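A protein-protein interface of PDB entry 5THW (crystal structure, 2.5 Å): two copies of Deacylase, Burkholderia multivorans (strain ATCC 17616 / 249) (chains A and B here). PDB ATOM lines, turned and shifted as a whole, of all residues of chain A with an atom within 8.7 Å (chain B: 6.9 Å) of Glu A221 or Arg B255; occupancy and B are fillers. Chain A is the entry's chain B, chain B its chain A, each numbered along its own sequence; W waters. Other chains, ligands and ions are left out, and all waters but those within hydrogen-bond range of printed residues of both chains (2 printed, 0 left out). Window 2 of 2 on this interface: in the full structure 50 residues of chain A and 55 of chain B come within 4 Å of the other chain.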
ATOM      1  N   GLU A 213      -9.606 -23.345  -3.392  1.00  0.00           N
ATOM      2  CA  GLU A 213     -10.379 -22.184  -2.953  1.00  0.00           C
ATOM      3  C   GLU A 213     -11.841 -22.261  -3.390  1.00  0.00           C
ATOM      4  O   GLU A 213     -12.726 -21.793  -2.665  1.00  0.00           O
ATOM      5  CB  GLU A 213      -9.727 -20.897  -3.470  1.00  0.00           C
ATOM      6  CG  GLU A 213     -10.403 -19.611  -3.015  1.00  0.00           C
ATOM      7  CD  GLU A 213      -9.951 -18.401  -3.813  1.00  0.00           C
ATOM      8  OE1 GLU A 213     -10.734 -17.430  -3.930  1.00  0.00           O
ATOM      9  OE2 GLU A 213      -8.799 -18.413  -4.301  1.00  0.00           O
ATOM     10  N   GLY A 215     -12.921 -20.470  -5.546  1.00  0.00           N
ATOM     11  CA  GLY A 215     -13.173 -19.092  -5.892  1.00  0.00           C
ATOM     12  C   GLY A 215     -11.977 -18.533  -6.623  1.00  0.00           C
ATOM     13  O   GLY A 215     -10.968 -19.219  -6.809  1.00  0.00           O
ATOM     14  N   PRO A 216     -12.064 -17.281  -7.063  1.00  0.00           N
ATOM     15  CA  PRO A 216     -11.033 -16.710  -7.948  1.00  0.00           C
ATOM     16  C   PRO A 216      -9.941 -15.885  -7.273  1.00  0.00           C
ATOM     17  O   PRO A 216      -9.043 -15.418  -7.985  1.00  0.00           O
ATOM     18  CB  PRO A 216     -11.877 -15.809  -8.853  1.00  0.00           C
ATOM     19  CG  PRO A 216     -12.906 -15.251  -7.891  1.00  0.00           C
ATOM     20  CD  PRO A 216     -13.212 -16.373  -6.903  1.00  0.00           C
ATOM     21  N   ILE A 217      -9.973 -15.710  -5.948  1.00  0.00           N
ATOM     22  CA  ILE A 217      -9.145 -14.684  -5.312  1.00  0.00           C
ATOM     23  C   ILE A 217      -7.663 -15.001  -5.482  1.00  0.00           C
ATOM     24  O   ILE A 217      -6.886 -14.171  -5.971  1.00  0.00           O
ATOM     25  CB  ILE A 217      -9.518 -14.530  -3.826  1.00  0.00           C
ATOM     26  CG1 ILE A 217     -10.990 -14.128  -3.674  1.00  0.00           C
ATOM     27  CG2 ILE A 217      -8.600 -13.513  -3.135  1.00  0.00           C
ATOM     28  CD1 ILE A 217     -11.405 -13.856  -2.233  1.00  0.00           C
ATOM     29  N   LEU A 218      -7.254 -16.213  -5.098  1.00  0.00           N
ATOM     30  CA  LEU A 218      -5.833 -16.543  -5.090  1.00  0.00           C
ATOM     31  C   LEU A 218      -5.244 -16.527  -6.498  1.00  0.00           C
ATOM     32  O   LEU A 218      -4.133 -16.023  -6.705  1.00  0.00           O
ATOM     33  CB  LEU A 218      -5.629 -17.910  -4.435  1.00  0.00           C
ATOM     34  CG  LEU A 218      -5.966 -17.996  -2.942  1.00  0.00           C
ATOM     35  CD1 LEU A 218      -5.857 -19.423  -2.427  1.00  0.00           C
ATOM     36  CD2 LEU A 218      -5.085 -17.058  -2.130  1.00  0.00           C
ATOM     37  N   GLU A 219      -5.983 -17.036  -7.482  1.00  0.00           N
ATOM     38  CA  GLU A 219      -5.491 -17.020  -8.856  1.00  0.00           C
ATOM     39  C   GLU A 219      -5.423 -15.601  -9.411  1.00  0.00           C
ATOM     40  O   GLU A 219      -4.429 -15.222 -10.043  1.00  0.00           O
ATOM     41  CB  GLU A 219      -6.371 -17.903  -9.738  1.00  0.00           C
ATOM     42  CG  GLU A 219      -5.903 -18.024 -11.183  1.00  0.00           C
ATOM     43  CD  GLU A 219      -6.982 -18.604 -12.084  1.00  0.00           C
ATOM     44  OE1 GLU A 219      -8.177 -18.355 -11.816  1.00  0.00           O
ATOM     45  OE2 GLU A 219      -6.641 -19.312 -13.056  1.00  0.00           O
ATOM     46  N   ALA A 220      -6.476 -14.805  -9.198  1.00  0.00           N
ATOM     47  CA  ALA A 220      -6.496 -13.448  -9.741  1.00  0.00           C
ATOM     48  C   ALA A 220      -5.356 -12.609  -9.180  1.00  0.00           C
ATOM     49  O   ALA A 220      -4.735 -11.824  -9.905  1.00  0.00           O
ATOM     50  CB  ALA A 220      -7.845 -12.776  -9.457  1.00  0.00           C
ATOM     51  N   GLU A 221      -5.062 -12.769  -7.895  1.00  0.00           N
ATOM     52  CA  GLU A 221      -4.026 -12.001  -7.223  1.00  0.00           C
ATOM     53  C   GLU A 221      -2.651 -12.650  -7.308  1.00  0.00           C
ATOM     54  O   GLU A 221      -1.719 -12.177  -6.649  1.00  0.00           O
ATOM     55  CB  GLU A 221      -4.415 -11.793  -5.765  1.00  0.00           C
ATOM     56  CG  GLU A 221      -5.716 -11.038  -5.624  1.00  0.00           C
ATOM     57  CD  GLU A 221      -6.048 -10.774  -4.184  1.00  0.00           C
ATOM     58  OE1 GLU A 221      -7.066 -10.102  -3.917  1.00  0.00           O
ATOM     59  OE2 GLU A 221      -5.281 -11.248  -3.320  1.00  0.00           O
ATOM     60  N   ARG A 222      -2.520 -13.737  -8.072  1.00  0.00           N
ATOM     61  CA  ARG A 222      -1.256 -14.459  -8.237  1.00  0.00           C
ATOM     62  C   ARG A 222      -0.638 -14.813  -6.886  1.00  0.00           C
ATOM     63  O   ARG A 222       0.561 -14.649  -6.658  1.00  0.00           O
ATOM     64  CB  ARG A 222      -0.288 -13.658  -9.109  1.00  0.00           C
ATOM     65  CG  ARG A 222      -0.965 -13.060 -10.327  1.00  0.00           C
ATOM     66  CD  ARG A 222      -0.020 -12.858 -11.496  1.00  0.00           C
ATOM     67  NE  ARG A 222      -0.579 -11.920 -12.469  1.00  0.00           N
ATOM     68  CZ  ARG A 222      -0.052 -11.666 -13.663  1.00  0.00           C
ATOM     69  NH1 ARG A 222       1.054 -12.287 -14.052  1.00  0.00           N
ATOM     70  NH2 ARG A 222      -0.637 -10.791 -14.472  1.00  0.00           N
ATOM     71  N   LYS A 223      -1.483 -15.269  -5.968  1.00  0.00           N
ATOM     72  CA  LYS A 223      -1.066 -15.753  -4.663  1.00  0.00           C
ATOM     73  C   LYS A 223      -1.170 -17.273  -4.664  1.00  0.00           C
ATOM     74  O   LYS A 223      -2.109 -17.833  -5.237  1.00  0.00           O
ATOM     75  CB  LYS A 223      -1.933 -15.143  -3.560  1.00  0.00           C
ATOM     76  CG  LYS A 223      -1.809 -13.620  -3.497  1.00  0.00           C
ATOM     77  CD  LYS A 223      -1.467 -13.109  -2.113  1.00  0.00           C
ATOM     78  CE  LYS A 223      -0.140 -12.368  -2.114  1.00  0.00           C
ATOM     79  NZ  LYS A 223      -0.085 -11.316  -3.158  1.00  0.00           N
ATOM     80  N   THR A 224      -0.192 -17.946  -4.057  1.00  0.00           N
ATOM     81  CA  THR A 224      -0.162 -19.406  -4.072  1.00  0.00           C
ATOM     82  C   THR A 224      -0.943 -20.030  -2.915  1.00  0.00           C
ATOM     83  O   THR A 224      -1.608 -21.054  -3.101  1.00  0.00           O
ATOM     84  CB  THR A 224       1.282 -19.912  -4.028  1.00  0.00           C
ATOM     85  OG1 THR A 224       1.992 -19.452  -5.181  1.00  0.00           O
ATOM     86  CG2 THR A 224       1.300 -21.420  -4.038  1.00  0.00           C
ATOM     87  N   ILE A 225      -0.893 -19.430  -1.728  1.00  0.00           N
ATOM     88  CA  ILE A 225      -1.477 -20.010  -0.525  1.00  0.00           C
ATOM     89  C   ILE A 225      -2.494 -19.041   0.060  1.00  0.00           C
ATOM     90  O   ILE A 225      -2.221 -17.843   0.184  1.00  0.00           O
ATOM     91  CB  ILE A 225      -0.394 -20.343   0.517  1.00  0.00           C
ATOM     92  CG1 ILE A 225       0.555 -21.410  -0.027  1.00  0.00           C
ATOM     93  CG2 ILE A 225      -1.030 -20.760   1.839  1.00  0.00           C
ATOM     94  CD1 ILE A 225      -0.118 -22.739  -0.255  1.00  0.00           C
ATOM     95  N   LEU A 275     -23.431  -5.406  -0.808  1.00  0.00           N
ATOM     96  CA  LEU A 275     -22.404  -4.373  -0.906  1.00  0.00           C
ATOM     97  C   LEU A 275     -22.358  -3.492   0.331  1.00  0.00           C
ATOM     98  O   LEU A 275     -21.301  -2.938   0.646  1.00  0.00           O
ATOM     99  CB  LEU A 275     -22.618  -3.511  -2.152  1.00  0.00           C
ATOM    100  CG  LEU A 275     -22.525  -4.186  -3.517  1.00  0.00           C
ATOM    101  CD1 LEU A 275     -22.895  -3.207  -4.593  1.00  0.00           C
ATOM    102  CD2 LEU A 275     -21.103  -4.701  -3.732  1.00  0.00           C
ATOM    103  N   PRO A 279     -16.088  -5.850   3.385  1.00  0.00           N
ATOM    104  CA  PRO A 279     -15.577  -6.487   2.167  1.00  0.00           C
ATOM    105  C   PRO A 279     -16.004  -7.931   1.957  1.00  0.00           C
ATOM    106  O   PRO A 279     -15.873  -8.427   0.843  1.00  0.00           O
ATOM    107  CB  PRO A 279     -14.069  -6.420   2.368  1.00  0.00           C
ATOM    108  CG  PRO A 279     -13.915  -6.594   3.827  1.00  0.00           C
ATOM    109  CD  PRO A 279     -15.077  -5.860   4.456  1.00  0.00           C
ATOM    110  N   PRO A 369       3.860 -16.819  -2.015  1.00  0.00           N
ATOM    111  CA  PRO A 369       3.001 -15.637  -1.835  1.00  0.00           C
ATOM    112  C   PRO A 369       1.640 -16.043  -1.279  1.00  0.00           C
ATOM    113  O   PRO A 369       1.004 -16.976  -1.769  1.00  0.00           O
ATOM    114  CB  PRO A 369       2.895 -15.048  -3.249  1.00  0.00           C
ATOM    115  CG  PRO A 369       3.418 -16.128  -4.181  1.00  0.00           C
ATOM    116  CD  PRO A 369       4.385 -16.938  -3.385  1.00  0.00           C
ATOM    117  N   HIS A 370       1.219 -15.369  -0.213  1.00  0.00           N
ATOM    118  CA  HIS A 370       0.037 -15.783   0.531  1.00  0.00           C
ATOM    119  C   HIS A 370      -0.759 -14.564   0.979  1.00  0.00           C
ATOM    120  O   HIS A 370      -0.285 -13.426   0.931  1.00  0.00           O
ATOM    121  CB  HIS A 370       0.407 -16.656   1.740  1.00  0.00           C
ATOM    122  CG  HIS A 370       1.320 -15.980   2.718  1.00  0.00           C
ATOM    123  ND1 HIS A 370       2.663 -15.786   2.473  1.00  0.00           N
ATOM    124  CD2 HIS A 370       1.076 -15.433   3.934  1.00  0.00           C
ATOM    125  CE1 HIS A 370       3.209 -15.159   3.501  1.00  0.00           C
ATOM    126  NE2 HIS A 370       2.268 -14.931   4.399  1.00  0.00           N
ATOM    127  N   ARG A 371      -1.990 -14.820   1.418  1.00  0.00           N
ATOM    128  CA  ARG A 371      -2.857 -13.783   1.963  1.00  0.00           C
ATOM    129  C   ARG A 371      -3.904 -14.432   2.849  1.00  0.00           C
ATOM    130  O   ARG A 371      -4.269 -15.592   2.655  1.00  0.00           O
ATOM    131  CB  ARG A 371      -3.549 -12.974   0.862  1.00  0.00           C
ATOM    132  CG  ARG A 371      -4.392 -13.814  -0.074  1.00  0.00           C
ATOM    133  CD  ARG A 371      -5.442 -12.961  -0.740  1.00  0.00           C
ATOM    134  NE  ARG A 371      -6.563 -12.702   0.147  1.00  0.00           N
ATOM    135  CZ  ARG A 371      -7.482 -11.769  -0.066  1.00  0.00           C
ATOM    136  NH1 ARG A 371      -7.398 -10.989  -1.132  1.00  0.00           N
ATOM    137  NH2 ARG A 371      -8.480 -11.611   0.794  1.00  0.00           N
ATOM    138  N   ASP A 372      -4.385 -13.665   3.822  1.00  0.00           N
ATOM    139  CA  ASP A 372      -5.490 -14.117   4.654  1.00  0.00           C
ATOM    140  C   ASP A 372      -6.758 -14.149   3.820  1.00  0.00           C
ATOM    141  O   ASP A 372      -7.014 -13.244   3.020  1.00  0.00           O
ATOM    142  CB  ASP A 372      -5.669 -13.189   5.857  1.00  0.00           C
ATOM    143  CG  ASP A 372      -4.531 -13.304   6.870  1.00  0.00           C
ATOM    144  OD1 ASP A 372      -3.568 -14.072   6.630  1.00  0.00           O
ATOM    145  OD2 ASP A 372      -4.590 -12.598   7.903  1.00  0.00           O
ATOM    146  N   ILE A 373      -7.551 -15.200   3.994  1.00  0.00           N
ATOM    147  CA  ILE A 373      -8.736 -15.387   3.174  1.00  0.00           C
ATOM    148  C   ILE A 373      -9.845 -15.983   4.030  1.00  0.00           C
ATOM    149  O   ILE A 373      -9.600 -16.765   4.956  1.00  0.00           O
ATOM    150  CB  ILE A 373      -8.420 -16.265   1.927  1.00  0.00           C
ATOM    151  CG1 ILE A 373      -9.550 -16.200   0.904  1.00  0.00           C
ATOM    152  CG2 ILE A 373      -8.158 -17.711   2.304  1.00  0.00           C
ATOM    153  CD1 ILE A 373      -9.095 -16.577  -0.479  1.00  0.00           C
ATOM    154  N   PRO A 396      -5.125 -22.032  -5.147  1.00  0.00           N
ATOM    155  CA  PRO A 396      -6.042 -21.511  -6.170  1.00  0.00           C
ATOM    156  C   PRO A 396      -6.596 -22.631  -7.038  1.00  0.00           C
ATOM    157  O   PRO A 396      -6.154 -23.782  -7.004  1.00  0.00           O
ATOM    158  CB  PRO A 396      -5.189 -20.540  -6.989  1.00  0.00           C
ATOM    159  CG  PRO A 396      -3.774 -20.855  -6.655  1.00  0.00           C
ATOM    160  CD  PRO A 396      -3.713 -21.728  -5.442  1.00  0.00           C
ATOM    161  N   GLN B 244     -20.598 -13.848 -15.857  1.00  0.00           N
ATOM    162  CA  GLN B 244     -19.676 -14.901 -15.468  1.00  0.00           C
ATOM    163  C   GLN B 244     -20.359 -15.721 -14.392  1.00  0.00           C
ATOM    164  O   GLN B 244     -20.658 -15.206 -13.310  1.00  0.00           O
ATOM    165  CB  GLN B 244     -18.349 -14.322 -14.956  1.00  0.00           C
ATOM    166  CG  GLN B 244     -17.287 -15.366 -14.611  1.00  0.00           C
ATOM    167  CD  GLN B 244     -17.142 -16.437 -15.680  1.00  0.00           C
ATOM    168  OE1 GLN B 244     -16.644 -16.179 -16.780  1.00  0.00           O
ATOM    169  NE2 GLN B 244     -17.584 -17.650 -15.362  1.00  0.00           N
ATOM    170  N   ALA B 246     -20.419 -18.227 -11.452  1.00  0.00           N
ATOM    171  CA  ALA B 246     -19.453 -18.535 -10.406  1.00  0.00           C
ATOM    172  C   ALA B 246     -20.210 -18.836  -9.121  1.00  0.00           C
ATOM    173  O   ALA B 246     -21.385 -18.492  -8.981  1.00  0.00           O
ATOM    174  CB  ALA B 246     -18.464 -17.382 -10.193  1.00  0.00           C
ATOM    175  N   PRO B 250     -17.720 -18.322  -2.496  1.00  0.00           N
ATOM    176  CA  PRO B 250     -16.315 -17.897  -2.563  1.00  0.00           C
ATOM    177  C   PRO B 250     -16.031 -16.806  -3.585  1.00  0.00           C
ATOM    178  O   PRO B 250     -14.891 -16.327  -3.634  1.00  0.00           O
ATOM    179  CB  PRO B 250     -15.569 -19.193  -2.938  1.00  0.00           C
ATOM    180  CG  PRO B 250     -16.606 -20.132  -3.430  1.00  0.00           C
ATOM    181  CD  PRO B 250     -17.900 -19.752  -2.806  1.00  0.00           C
ATOM    182  N   THR B 251     -17.005 -16.371  -4.396  1.00  0.00           N
ATOM    183  CA  THR B 251     -16.776 -15.248  -5.304  1.00  0.00           C
ATOM    184  C   THR B 251     -17.100 -13.932  -4.600  1.00  0.00           C
ATOM    185  O   THR B 251     -18.278 -13.673  -4.311  1.00  0.00           O
ATOM    186  CB  THR B 251     -17.612 -15.382  -6.572  1.00  0.00           C
ATOM    187  OG1 THR B 251     -17.382 -16.658  -7.180  1.00  0.00           O
ATOM    188  CG2 THR B 251     -17.230 -14.295  -7.566  1.00  0.00           C
ATOM    189  N   PRO B 252     -16.118 -13.084  -4.313  1.00  0.00           N
ATOM    190  CA  PRO B 252     -16.409 -11.818  -3.631  1.00  0.00           C
ATOM    191  C   PRO B 252     -17.181 -10.863  -4.534  1.00  0.00           C
ATOM    192  O   PRO B 252     -17.108 -10.935  -5.765  1.00  0.00           O
ATOM    193  CB  PRO B 252     -15.024 -11.264  -3.272  1.00  0.00           C
ATOM    194  CG  PRO B 252     -14.073 -11.934  -4.178  1.00  0.00           C
ATOM    195  CD  PRO B 252     -14.709 -13.196  -4.721  1.00  0.00           C
ATOM    196  N   MET B 253     -17.971 -10.000  -3.894  1.00  0.00           N
ATOM    197  CA  MET B 253     -18.830  -9.061  -4.616  1.00  0.00           C
ATOM    198  C   MET B 253     -18.096  -8.203  -5.649  1.00  0.00           C
ATOM    199  O   MET B 253     -18.671  -7.973  -6.726  1.00  0.00           O
ATOM    200  CB  MET B 253     -19.568  -8.157  -3.614  1.00  0.00           C
ATOM    201  CG  MET B 253     -20.572  -8.873  -2.724  1.00  0.00           C
ATOM    202  SD  MET B 253     -21.946  -9.612  -3.629  1.00  0.00           S
ATOM    203  CE  MET B 253     -22.985  -8.158  -3.841  1.00  0.00           C
ATOM    204  N   PRO B 254     -16.894  -7.667  -5.400  1.00  0.00           N
ATOM    205  CA  PRO B 254     -16.256  -6.833  -6.435  1.00  0.00           C
ATOM    206  C   PRO B 254     -15.931  -7.580  -7.723  1.00  0.00           C
ATOM    207  O   PRO B 254     -15.759  -6.934  -8.763  1.00  0.00           O
ATOM    208  CB  PRO B 254     -14.984  -6.311  -5.747  1.00  0.00           C
ATOM    209  CG  PRO B 254     -15.258  -6.416  -4.295  1.00  0.00           C
ATOM    210  CD  PRO B 254     -16.132  -7.628  -4.137  1.00  0.00           C
ATOM    211  N   ARG B 255     -15.799  -8.910  -7.684  1.00  0.00           N
ATOM    212  CA  ARG B 255     -15.396  -9.702  -8.843  1.00  0.00           C
ATOM    213  C   ARG B 255     -16.577 -10.293  -9.634  1.00  0.00           C
ATOM    214  O   ARG B 255     -16.377 -11.257 -10.382  1.00  0.00           O
ATOM    215  CB  ARG B 255     -14.448 -10.823  -8.403  1.00  0.00           C
ATOM    216  CG  ARG B 255     -13.252 -10.330  -7.586  1.00  0.00           C
ATOM    217  CD  ARG B 255     -12.200 -11.408  -7.367  1.00  0.00           C
ATOM    218  NE  ARG B 255     -11.051 -10.891  -6.627  1.00  0.00           N
ATOM    219  CZ  ARG B 255     -10.044 -10.216  -7.175  1.00  0.00           C
ATOM    220  NH1 ARG B 255     -10.046  -9.960  -8.477  1.00  0.00           N
ATOM    221  NH2 ARG B 255      -9.041  -9.780  -6.419  1.00  0.00           N
ATOM    222  N   ARG B 256     -17.797  -9.777  -9.463  1.00  0.00           N
ATOM    223  CA  ARG B 256     -18.974 -10.386 -10.070  1.00  0.00           C
ATOM    224  C   ARG B 256     -19.406  -9.716 -11.370  1.00  0.00           C
ATOM    225  O   ARG B 256     -19.295  -8.502 -11.539  1.00  0.00           O
ATOM    226  CB  ARG B 256     -20.144 -10.395  -9.091  1.00  0.00           C
ATOM    227  CG  ARG B 256     -19.816 -11.165  -7.835  1.00  0.00           C
ATOM    228  CD  ARG B 256     -20.996 -11.302  -6.907  1.00  0.00           C
ATOM    229  NE  ARG B 256     -20.679 -12.189  -5.792  1.00  0.00           N
ATOM    230  CZ  ARG B 256     -21.584 -12.866  -5.096  1.00  0.00           C
ATOM    231  NH1 ARG B 256     -22.871 -12.808  -5.427  1.00  0.00           N
ATOM    232  NH2 ARG B 256     -21.193 -13.629  -4.085  1.00  0.00           N
ATOM    233  N   ARG B 257     -19.923 -10.543 -12.290  1.00  0.00           N
ATOM    234  CA  ARG B 257     -20.638 -10.109 -13.496  1.00  0.00           C
ATOM    235  C   ARG B 257     -21.957 -10.892 -13.509  1.00  0.00           C
ATOM    236  O   ARG B 257     -22.115 -11.875 -14.241  1.00  0.00           O
ATOM    237  CB  ARG B 257     -19.803 -10.334 -14.773  1.00  0.00           C
ATOM    238  CG  ARG B 257     -18.435  -9.674 -14.726  1.00  0.00           C
ATOM    239  CD  ARG B 257     -17.808  -9.478 -16.099  1.00  0.00           C
ATOM    240  NE  ARG B 257     -17.359 -10.722 -16.716  1.00  0.00           N
ATOM    241  CZ  ARG B 257     -17.817 -11.206 -17.869  1.00  0.00           C
ATOM    242  NH1 ARG B 257     -18.745 -10.550 -18.555  1.00  0.00           N
ATOM    243  NH2 ARG B 257     -17.332 -12.349 -18.346  1.00  0.00           N
ATOM    244  N   ILE B 298     -23.986 -17.547  -8.990  1.00  0.00           N
ATOM    245  CA  ILE B 298     -24.248 -16.292  -9.699  1.00  0.00           C
ATOM    246  C   ILE B 298     -24.685 -16.619 -11.124  1.00  0.00           C
ATOM    247  O   ILE B 298     -23.997 -17.390 -11.821  1.00  0.00           O
ATOM    248  CB  ILE B 298     -22.981 -15.419  -9.708  1.00  0.00           C
ATOM    249  CG1 ILE B 298     -22.516 -15.138  -8.277  1.00  0.00           C
ATOM    250  CG2 ILE B 298     -23.229 -14.142 -10.493  1.00  0.00           C
ATOM    251  CD1 ILE B 298     -21.040 -14.801  -8.169  1.00  0.00           C
HETATM  252  O   HOH W   1     -12.870 -17.028  -2.104  1.00  0.00           O
HETATM  253  O   HOH W   2     -17.587  -9.814  -0.775  1.00  0.00           O
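OE1 of Glu A221 lies within salt-bridge range of NH2 of Arg B255.
The side-chain sulfur (SD) of Met B253 lies close to the guanidinium group (NE) of Arg B256, at 3.6 Å.
The backbone NH (N) of Ile A217 lies within hydrogen-bond range of the side-chain carboxylate (OE1) of Glu A213 (2.8 Å).
N of Leu A218 sits at hydrogen-bond distance from OE2 of Glu A213 (2.8 Å).
The side-chain carboxylate of Glu A221 is in salt-bridge range of the guanidinium group of Arg A371, at 2.9 Å.
Glu A213 touches Pro B250.
Gly A215 touches Pro B250.
Pro A216 touches Pro B250.
Pro A216 touches Arg B255 (CG to CD, 3.9 Å).
Ile A217 touches Pro B252.
Ala A220 touches Arg B255 (CB to NH1, 3.7 Å).
Met B253 touches Leu A275.
Of the printed residues of chain B, Glu A213 touches Pro B250.
Of the printed residues of chain B, Ile A217 touches Pro B252.
Of the printed residues of chain B, Ala A220 touches Arg B255 (3.7 Å).
Glu A221 touches one residue of chain B.
No residue of chain A comes within 4 Å of Pro B254.
The nearest residue of chain A that does not touch Arg B255 is Ile A217 (4.4 Å).
The nearest printed residue of chain B that does not touch Leu A275 is Pro B254 (5.4 Å).
Hydrophobic or aromatic side chains of chain A within 4 Å of the printed part of chain B: Pro A216, Ile A217, Ala A220 and Leu A275.
Among the printed residues, Asp or Glu carboxylates within 4 Å of a Lys or Arg side-chain nitrogen of the other chain: Glu A221 with Arg B255 (3.2 Å).
No position is printed for both chains.
Of the 8 pairs that touch across the chains among the printed residues, none has its exchanged pair printed and touching as well.
Water W1 lies within hydrogen-bond range of the backbone carbonyl oxygen of Pro B250 (2.6 Å) and the side-chain carboxylate of Glu A213 (2.8 Å).
Water W2 lies within hydrogen-bond range of O of Pro A279 (2.7 Å) and N of Met B253 (3.1 Å).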
